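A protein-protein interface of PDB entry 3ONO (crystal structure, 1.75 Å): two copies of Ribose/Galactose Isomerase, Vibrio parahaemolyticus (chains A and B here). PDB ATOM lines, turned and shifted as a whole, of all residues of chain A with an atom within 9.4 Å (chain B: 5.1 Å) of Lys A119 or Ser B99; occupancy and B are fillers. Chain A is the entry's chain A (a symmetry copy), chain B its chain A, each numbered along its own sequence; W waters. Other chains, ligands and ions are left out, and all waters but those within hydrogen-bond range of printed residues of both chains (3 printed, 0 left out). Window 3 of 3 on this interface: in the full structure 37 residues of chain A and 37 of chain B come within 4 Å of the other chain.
The side-chain hydroxyl (OH) of Tyr B94 is in hydrogen-bond range of the backbone carbonyl oxygen (O) of Thr A76 (2.6 Å). The side-chain amide nitrogen (NE2) of Gln A78 lies within hydrogen-bond range of the backbone carbonyl oxygen (O) of Tyr B94 (2.8 Å). The side-chain carboxylate of Glu B97 lies within salt-bridge range of the side-chain amino group of Lys A119 (2.6 Å). OD1 of Asp B100 lies within salt-bridge range of NZ of Lys A119.
OE2 of Glu B97 is in hydrogen-bond range of OG of Ser B99. OD2 of Asp B100 sits at hydrogen-bond distance from N of Glu B97 (3.1 Å). The backbone carbonyl oxygen (O) of Gly A75 lies within hydrogen-bond range of the backbone NH (N) of Lys A119, 2.9 Å away. The backbone NH (N) of Gln A78 lies close to the side-chain hydroxyl (OG1) of Thr A76. O of Leu A96 lies within hydrogen-bond range of ND2 of Asn A128 (2.9 Å).
Leu A96 touches Tyr B94 (CD1 to CE1, 3.9 Å). Lys A119 touches Ser B99. Leu B103 touches Lys A119 (CD1 to CG, 3.8 Å).
Of the printed residues of chain B, Lys A119 touches Glu B97, Ser B99, Asp B100 and Leu B103. No residue of chain A comes within 4 Å of Pro B98. Of chain A, only Lys A119 (2.8 Å) comes within 4 Å of Asp B100. No residue of chain A comes within 4 Å of Ala B101. Of the printed residues of chain B, Leu A96 touches Tyr B94 (3.9 Å). Of the printed residues of chain A, Leu B103 touches Lys A119 (3.8 Å). Printed residues of chain B within 4 Å of Thr A76: Tyr B94 (2.6 Å). Printed residues of chain B within 4 Å of Gln A78: Tyr B94. Printed residues of chain A within 4 Å of Glu B97: Lys A119 (2.6 Å). Leu A115 touches none of the printed residues of chain B. Lys A17 touches none of the printed residues of chain B.
Of the 20 printed residues of chain A, 4 touch a printed residue of chain B. Hydrophobic or aromatic side chains of chain A within 4 Å of the printed part of chain B: Leu A96. Hydrophobic or aromatic side chains of chain B that line the printed part of chain A: Tyr B94 and Leu B103. Among the printed residues, 7 pairs touch across the chains. Among the printed residues, Asp or Glu carboxylates within 4 Å of a Lys or Arg side-chain nitrogen of the other chain: Lys A119 with Glu B97 and Lys A119 with Asp B100.
No position is printed for both chains. Of the 7 pairs that touch across the chains among the printed residues, none has its exchanged pair printed and touching as well.
Water W1 lies within hydrogen-bond range of OD2 of Asp B100 (2.6 Å) and NZ of Lys A119 (3.4 Å). Water W3 lies within hydrogen-bond range of O of Asp B100, NE2 of Gln A78 and N of Phe B104. Water W2 lies within hydrogen-bond range of the side-chain hydroxyl of Tyr B94 (3.0 Å) and the side-chain amino group of Lys A119 (3.0 Å).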
ATOM      1  N   SER A  13       9.364   4.201  -5.178  1.00  0.00           N
ATOM      2  CA  SER A  13       9.551   4.379  -6.623  1.00  0.00           C
ATOM      3  C   SER A  13       9.810   3.047  -7.338  1.00  0.00           C
ATOM      4  O   SER A  13       9.449   2.875  -8.514  1.00  0.00           O
ATOM      5  CB  SER A  13      10.649   5.412  -6.950  1.00  0.00           C
ATOM      6  OG  SER A  13      11.968   4.920  -6.724  1.00  0.00           O
ATOM      7  N   GLN A  14      10.419   2.103  -6.625  1.00  0.00           N
ATOM      8  CA  GLN A  14      10.767   0.803  -7.216  1.00  0.00           C
ATOM      9  C   GLN A  14       9.965  -0.371  -6.646  1.00  0.00           C
ATOM     10  O   GLN A  14      10.302  -1.530  -6.878  1.00  0.00           O
ATOM     11  CB  GLN A  14      12.260   0.529  -7.033  1.00  0.00           C
ATOM     12  CG  GLN A  14      13.130   1.679  -7.479  1.00  0.00           C
ATOM     13  CD  GLN A  14      12.848   2.079  -8.918  1.00  0.00           C
ATOM     14  OE1 GLN A  14      12.790   1.228  -9.814  1.00  0.00           O
ATOM     15  NE2 GLN A  14      12.656   3.379  -9.146  1.00  0.00           N
ATOM     16  N   LYS A  17       8.862  -3.595  -8.396  1.00  0.00           N
ATOM     17  CA  LYS A  17       9.904  -4.565  -8.699  1.00  0.00           C
ATOM     18  C   LYS A  17      10.304  -5.429  -7.520  1.00  0.00           C
ATOM     19  O   LYS A  17      11.164  -6.309  -7.664  1.00  0.00           O
ATOM     20  CB  LYS A  17      11.137  -3.860  -9.268  1.00  0.00           C
ATOM     21  CG  LYS A  17      10.936  -3.424 -10.703  1.00  0.00           C
ATOM     22  CD  LYS A  17      12.057  -2.545 -11.246  1.00  0.00           C
ATOM     23  CE  LYS A  17      11.821  -2.291 -12.733  1.00  0.00           C
ATOM     24  NZ  LYS A  17      12.765  -1.286 -13.303  1.00  0.00           N
ATOM     25  N   CYS A  74      17.269   1.961  -5.159  1.00  0.00           N
ATOM     26  CA  CYS A  74      16.168   2.804  -5.605  1.00  0.00           C
ATOM     27  C   CYS A  74      16.370   2.958  -7.112  1.00  0.00           C
ATOM     28  O   CYS A  74      16.990   2.080  -7.729  1.00  0.00           O
ATOM     29  CB  CYS A  74      16.118   4.140  -4.837  1.00  0.00           C
ATOM     30  SG  CYS A  74      17.700   5.026  -4.707  1.00  0.00           S
ATOM     31  N   GLY A  75      15.843   4.012  -7.733  1.00  0.00           N
ATOM     32  CA  GLY A  75      15.946   4.101  -9.201  1.00  0.00           C
ATOM     33  C   GLY A  75      17.396   4.074  -9.671  1.00  0.00           C
ATOM     34  O   GLY A  75      17.765   3.337 -10.584  1.00  0.00           O
ATOM     35  N   THR A  76      18.241   4.891  -9.045  1.00  0.00           N
ATOM     36  CA  THR A  76      19.659   4.910  -9.395  1.00  0.00           C
ATOM     37  C   THR A  76      20.526   4.301  -8.292  1.00  0.00           C
ATOM     38  O   THR A  76      21.719   4.102  -8.503  1.00  0.00           O
ATOM     39  CB  THR A  76      20.168   6.348  -9.617  1.00  0.00           C
ATOM     40  OG1 THR A  76      20.056   7.074  -8.387  1.00  0.00           O
ATOM     41  CG2 THR A  76      19.330   7.063 -10.680  1.00  0.00           C
ATOM     42  N   GLY A  77      19.938   4.044  -7.118  1.00  0.00           N
ATOM     43  CA  GLY A  77      20.704   3.598  -5.957  1.00  0.00           C
ATOM     44  C   GLY A  77      21.328   4.716  -5.126  1.00  0.00           C
ATOM     45  O   GLY A  77      21.779   4.477  -3.994  1.00  0.00           O
ATOM     46  N   GLN A  78      21.372   5.932  -5.672  1.00  0.00           N
ATOM     47  CA  GLN A  78      22.075   7.035  -4.996  1.00  0.00           C
ATOM     48  C   GLN A  78      21.413   7.473  -3.686  1.00  0.00           C
ATOM     49  O   GLN A  78      22.080   7.575  -2.656  1.00  0.00           O
ATOM     50  CB  GLN A  78      22.205   8.250  -5.919  1.00  0.00           C
ATOM     51  CG  GLN A  78      22.935   7.956  -7.255  1.00  0.00           C
ATOM     52  CD  GLN A  78      24.429   8.220  -7.163  1.00  0.00           C
ATOM     53  OE1 GLN A  78      25.043   7.970  -6.116  1.00  0.00           O
ATOM     54  NE2 GLN A  78      25.034   8.691  -8.270  1.00  0.00           N
ATOM     55  N   CYS A  95      26.179  -1.159  -5.972  1.00  0.00           N
ATOM     56  CA  CYS A  95      26.382  -2.441  -6.618  1.00  0.00           C
ATOM     57  C   CYS A  95      25.615  -2.447  -7.914  1.00  0.00           C
ATOM     58  O   CYS A  95      24.394  -2.542  -7.896  1.00  0.00           O
ATOM     59  CB  CYS A  95      25.878  -3.559  -5.716  1.00  0.00           C
ATOM     60  SG  CYS A  95      26.564  -5.116  -6.208  1.00  0.00           S
ATOM     61  N   LEU A  96      26.334  -2.343  -9.029  1.00  0.00           N
ATOM     62  CA  LEU A  96      25.702  -2.215 -10.339  1.00  0.00           C
ATOM     63  C   LEU A  96      25.917  -3.423 -11.246  1.00  0.00           C
ATOM     64  O   LEU A  96      25.168  -3.637 -12.195  1.00  0.00           O
ATOM     65  CB  LEU A  96      26.223  -0.956 -11.032  1.00  0.00           C
ATOM     66  CG  LEU A  96      25.956   0.329 -10.242  1.00  0.00           C
ATOM     67  CD1 LEU A  96      26.535   1.503 -11.008  1.00  0.00           C
ATOM     68  CD2 LEU A  96      24.465   0.532  -9.994  1.00  0.00           C
ATOM     69  N   LEU A 115      21.421  -1.119  -4.952  1.00  0.00           N
ATOM     70  CA  LEU A 115      21.323  -1.414  -6.378  1.00  0.00           C
ATOM     71  C   LEU A 115      20.529  -0.346  -7.103  1.00  0.00           C
ATOM     72  O   LEU A 115      19.746   0.371  -6.483  1.00  0.00           O
ATOM     73  CB  LEU A 115      20.609  -2.761  -6.577  1.00  0.00           C
ATOM     74  CG  LEU A 115      21.455  -4.029  -6.381  1.00  0.00           C
ATOM     75  CD1 LEU A 115      21.933  -4.164  -4.925  1.00  0.00           C
ATOM     76  CD2 LEU A 115      20.645  -5.275  -6.780  1.00  0.00           C
ATOM     77  N   ALA A 116      20.715  -0.274  -8.422  1.00  0.00           N
ATOM     78  CA  ALA A 116      19.892   0.593  -9.270  1.00  0.00           C
ATOM     79  C   ALA A 116      18.838  -0.278  -9.934  1.00  0.00           C
ATOM     80  O   ALA A 116      19.178  -1.193 -10.701  1.00  0.00           O
ATOM     81  CB  ALA A 116      20.768   1.266 -10.327  1.00  0.00           C
ATOM     82  N   PHE A 117      17.569  -0.016  -9.639  1.00  0.00           N
ATOM     83  CA  PHE A 117      16.484  -0.838 -10.172  1.00  0.00           C
ATOM     84  C   PHE A 117      15.787  -0.205 -11.380  1.00  0.00           C
ATOM     85  O   PHE A 117      14.941  -0.851 -11.997  1.00  0.00           O
ATOM     86  CB  PHE A 117      15.443  -1.145  -9.090  1.00  0.00           C
ATOM     87  CG  PHE A 117      15.997  -1.902  -7.914  1.00  0.00           C
ATOM     88  CD1 PHE A 117      16.531  -3.171  -8.081  1.00  0.00           C
ATOM     89  CD2 PHE A 117      15.997  -1.344  -6.653  1.00  0.00           C
ATOM     90  CE1 PHE A 117      17.040  -3.861  -6.998  1.00  0.00           C
ATOM     91  CE2 PHE A 117      16.506  -2.043  -5.564  1.00  0.00           C
ATOM     92  CZ  PHE A 117      17.031  -3.304  -5.762  1.00  0.00           C
ATOM     93  N   ALA A 118      16.121   1.045 -11.712  1.00  0.00           N
ATOM     94  CA  ALA A 118      15.504   1.704 -12.872  1.00  0.00           C
ATOM     95  C   ALA A 118      16.534   2.142 -13.899  1.00  0.00           C
ATOM     96  O   ALA A 118      16.434   1.781 -15.069  1.00  0.00           O
ATOM     97  CB  ALA A 118      14.635   2.891 -12.429  1.00  0.00           C
ATOM     98  N   LYS A 119      17.521   2.916 -13.474  1.00  0.00           N
ATOM     99  CA  LYS A 119      18.566   3.370 -14.387  1.00  0.00           C
ATOM    100  C   LYS A 119      19.450   2.183 -14.785  1.00  0.00           C
ATOM    101  O   LYS A 119      19.946   1.450 -13.928  1.00  0.00           O
ATOM    102  CB  LYS A 119      19.394   4.457 -13.707  1.00  0.00           C
ATOM    103  CG  LYS A 119      20.344   5.207 -14.631  1.00  0.00           C
ATOM    104  CD  LYS A 119      21.753   4.751 -14.464  1.00  0.00           C
ATOM    105  CE  LYS A 119      22.697   5.600 -15.288  1.00  0.00           C
ATOM    106  NZ  LYS A 119      23.987   4.909 -15.359  1.00  0.00           N
ATOM    107  N   GLY A 120      19.667   1.997 -16.079  1.00  0.00           N
ATOM    108  CA  GLY A 120      20.415   0.841 -16.549  1.00  0.00           C
ATOM    109  C   GLY A 120      19.659  -0.480 -16.463  1.00  0.00           C
ATOM    110  O   GLY A 120      20.234  -1.541 -16.733  1.00  0.00           O
ATOM    111  N   PHE A 121      18.389  -0.435 -16.073  1.00  0.00           N
ATOM    112  CA  PHE A 121      17.622  -1.658 -15.847  1.00  0.00           C
ATOM    113  C   PHE A 121      16.618  -1.817 -16.948  1.00  0.00           C
ATOM    114  O   PHE A 121      15.562  -1.177 -16.953  1.00  0.00           O
ATOM    115  CB  PHE A 121      16.872  -1.633 -14.494  1.00  0.00           C
ATOM    116  CG  PHE A 121      16.301  -2.978 -14.106  1.00  0.00           C
ATOM    117  CD1 PHE A 121      16.950  -3.766 -13.163  1.00  0.00           C
ATOM    118  CD2 PHE A 121      15.155  -3.474 -14.711  1.00  0.00           C
ATOM    119  CE1 PHE A 121      16.446  -5.005 -12.804  1.00  0.00           C
ATOM    120  CE2 PHE A 121      14.654  -4.725 -14.369  1.00  0.00           C
ATOM    121  CZ  PHE A 121      15.306  -5.489 -13.413  1.00  0.00           C
ATOM    122  N   GLY A 122      16.936  -2.691 -17.881  1.00  0.00           N
ATOM    123  CA  GLY A 122      16.033  -2.891 -18.981  1.00  0.00           C
ATOM    124  C   GLY A 122      15.762  -4.346 -19.131  1.00  0.00           C
ATOM    125  O   GLY A 122      15.655  -5.088 -18.171  1.00  0.00           O
ATOM    126  N   GLY A 125      17.213  -7.240 -17.033  1.00  0.00           N
ATOM    127  CA  GLY A 125      17.752  -6.648 -15.811  1.00  0.00           C
ATOM    128  C   GLY A 125      17.750  -7.608 -14.626  1.00  0.00           C
ATOM    129  O   GLY A 125      18.614  -7.539 -13.752  1.00  0.00           O
ATOM    130  N   ASN A 128      21.042  -9.632 -14.136  1.00  0.00           N
ATOM    131  CA  ASN A 128      22.092  -8.901 -13.437  1.00  0.00           C
ATOM    132  C   ASN A 128      21.842  -8.898 -11.916  1.00  0.00           C
ATOM    133  O   ASN A 128      22.773  -9.073 -11.126  1.00  0.00           O
ATOM    134  CB  ASN A 128      22.192  -7.486 -14.004  1.00  0.00           C
ATOM    135  CG  ASN A 128      23.361  -6.717 -13.441  1.00  0.00           C
ATOM    136  OD1 ASN A 128      24.511  -7.131 -13.587  1.00  0.00           O
ATOM    137  ND2 ASN A 128      23.076  -5.574 -12.809  1.00  0.00           N
ATOM    138  N   TYR B  94      27.893   8.221  -6.336  1.00  0.00           N
ATOM    139  CA  TYR B  94      28.858   7.566  -7.223  1.00  0.00           C
ATOM    140  C   TYR B  94      28.761   8.216  -8.602  1.00  0.00           C
ATOM    141  O   TYR B  94      27.745   8.808  -8.949  1.00  0.00           O
ATOM    142  CB  TYR B  94      28.606   6.040  -7.319  1.00  0.00           C
ATOM    143  CG  TYR B  94      27.324   5.639  -8.025  1.00  0.00           C
ATOM    144  CD1 TYR B  94      27.238   5.665  -9.424  1.00  0.00           C
ATOM    145  CD2 TYR B  94      26.196   5.228  -7.310  1.00  0.00           C
ATOM    146  CE1 TYR B  94      26.052   5.312 -10.099  1.00  0.00           C
ATOM    147  CE2 TYR B  94      25.003   4.855  -7.982  1.00  0.00           C
ATOM    148  CZ  TYR B  94      24.947   4.903  -9.365  1.00  0.00           C
ATOM    149  OH  TYR B  94      23.784   4.566 -10.026  1.00  0.00           O
ATOM    150  N   GLU B  97      29.715   6.964 -15.162  1.00  0.00           N
ATOM    151  CA  GLU B  97      29.539   7.252 -16.595  1.00  0.00           C
ATOM    152  C   GLU B  97      28.744   8.557 -16.639  1.00  0.00           C
ATOM    153  O   GLU B  97      28.124   8.934 -15.643  1.00  0.00           O
ATOM    154  CB  GLU B  97      28.860   6.084 -17.303  1.00  0.00           C
ATOM    155  CG  GLU B  97      27.490   5.722 -16.758  1.00  0.00           C
ATOM    156  CD  GLU B  97      26.402   6.453 -17.519  1.00  0.00           C
ATOM    157  OE1 GLU B  97      26.753   7.230 -18.433  1.00  0.00           O
ATOM    158  OE2 GLU B  97      25.210   6.253 -17.224  1.00  0.00           O
ATOM    159  N   PRO B  98      28.809   9.288 -17.748  1.00  0.00           N
ATOM    160  CA  PRO B  98      28.276  10.657 -17.802  1.00  0.00           C
ATOM    161  C   PRO B  98      26.833  10.857 -17.339  1.00  0.00           C
ATOM    162  O   PRO B  98      26.554  11.861 -16.682  1.00  0.00           O
ATOM    163  CB  PRO B  98      28.396  11.022 -19.281  1.00  0.00           C
ATOM    164  CG  PRO B  98      29.539  10.196 -19.751  1.00  0.00           C
ATOM    165  CD  PRO B  98      29.507   8.914 -18.997  1.00  0.00           C
ATOM    166  N   SER B  99      25.915   9.956 -17.668  1.00  0.00           N
ATOM    167  CA  SER B  99      24.532  10.218 -17.258  1.00  0.00           C
ATOM    168  C   SER B  99      24.328  10.079 -15.737  1.00  0.00           C
ATOM    169  O   SER B  99      23.335  10.575 -15.191  1.00  0.00           O
ATOM    170  CB  SER B  99      23.531   9.359 -18.038  1.00  0.00           C
ATOM    171  OG  SER B  99      23.326   8.112 -17.411  1.00  0.00           O
ATOM    172  N   ASP B 100      25.253   9.414 -15.046  1.00  0.00           N
ATOM    173  CA  ASP B 100      25.218   9.427 -13.569  1.00  0.00           C
ATOM    174  C   ASP B 100      25.308  10.843 -13.016  1.00  0.00           C
ATOM    175  O   ASP B 100      24.663  11.180 -12.019  1.00  0.00           O
ATOM    176  CB  ASP B 100      26.394   8.639 -12.960  1.00  0.00           C
ATOM    177  CG  ASP B 100      26.308   7.131 -13.224  1.00  0.00           C
ATOM    178  OD1 ASP B 100      25.199   6.613 -13.458  1.00  0.00           O
ATOM    179  OD2 ASP B 100      27.368   6.454 -13.156  1.00  0.00           O
ATOM    180  N   ALA B 101      26.182  11.649 -13.618  1.00  0.00           N
ATOM    181  CA  ALA B 101      26.455  12.995 -13.136  1.00  0.00           C
ATOM    182  C   ALA B 101      25.224  13.876 -13.334  1.00  0.00           C
ATOM    183  O   ALA B 101      24.821  14.627 -12.428  1.00  0.00           O
ATOM    184  CB  ALA B 101      27.646  13.595 -13.885  1.00  0.00           C
ATOM    185  N   PHE B 102      24.641  13.793 -14.522  1.00  0.00           N
ATOM    186  CA  PHE B 102      23.431  14.554 -14.794  1.00  0.00           C
ATOM    187  C   PHE B 102      22.298  14.191 -13.828  1.00  0.00           C
ATOM    188  O   PHE B 102      21.717  15.076 -13.190  1.00  0.00           O
ATOM    189  CB  PHE B 102      22.961  14.368 -16.220  1.00  0.00           C
ATOM    190  CG  PHE B 102      21.705  15.124 -16.516  1.00  0.00           C
ATOM    191  CD1 PHE B 102      21.739  16.499 -16.672  1.00  0.00           C
ATOM    192  CD2 PHE B 102      20.492  14.473 -16.563  1.00  0.00           C
ATOM    193  CE1 PHE B 102      20.578  17.202 -16.912  1.00  0.00           C
ATOM    194  CE2 PHE B 102      19.321  15.176 -16.813  1.00  0.00           C
ATOM    195  CZ  PHE B 102      19.365  16.528 -16.984  1.00  0.00           C
ATOM    196  N   LEU B 103      21.993  12.900 -13.719  1.00  0.00           N
ATOM    197  CA  LEU B 103      20.920  12.443 -12.830  1.00  0.00           C
ATOM    198  C   LEU B 103      21.214  12.796 -11.374  1.00  0.00           C
ATOM    199  O   LEU B 103      20.316  13.197 -10.632  1.00  0.00           O
ATOM    200  CB  LEU B 103      20.715  10.934 -12.944  1.00  0.00           C
ATOM    201  CG  LEU B 103      20.177  10.479 -14.301  1.00  0.00           C
ATOM    202  CD1 LEU B 103      20.167   8.968 -14.379  1.00  0.00           C
ATOM    203  CD2 LEU B 103      18.767  11.081 -14.509  1.00  0.00           C
ATOM    204  N   PHE B 104      22.460  12.628 -10.947  1.00  0.00           N
ATOM    205  CA  PHE B 104      22.804  12.996  -9.578  1.00  0.00           C
ATOM    206  C   PHE B 104      22.460  14.464  -9.324  1.00  0.00           C
ATOM    207  O   PHE B 104      21.822  14.802  -8.328  1.00  0.00           O
ATOM    208  CB  PHE B 104      24.288  12.762  -9.314  1.00  0.00           C
ATOM    209  CG  PHE B 104      24.747  13.200  -7.935  1.00  0.00           C
ATOM    210  CD1 PHE B 104      24.407  12.474  -6.807  1.00  0.00           C
ATOM    211  CD2 PHE B 104      25.536  14.333  -7.786  1.00  0.00           C
ATOM    212  CE1 PHE B 104      24.859  12.864  -5.552  1.00  0.00           C
ATOM    213  CE2 PHE B 104      25.983  14.731  -6.520  1.00  0.00           C
ATOM    214  CZ  PHE B 104      25.634  13.986  -5.414  1.00  0.00           C
HETATM  215  O   HOH W   1      26.740   3.946 -13.680  1.00  0.00           O
HETATM  216  O   HOH W   2      24.022   3.386 -12.735  1.00  0.00           O
HETATM  217  O   HOH W   3      23.119   9.347 -10.514  1.00  0.00           O
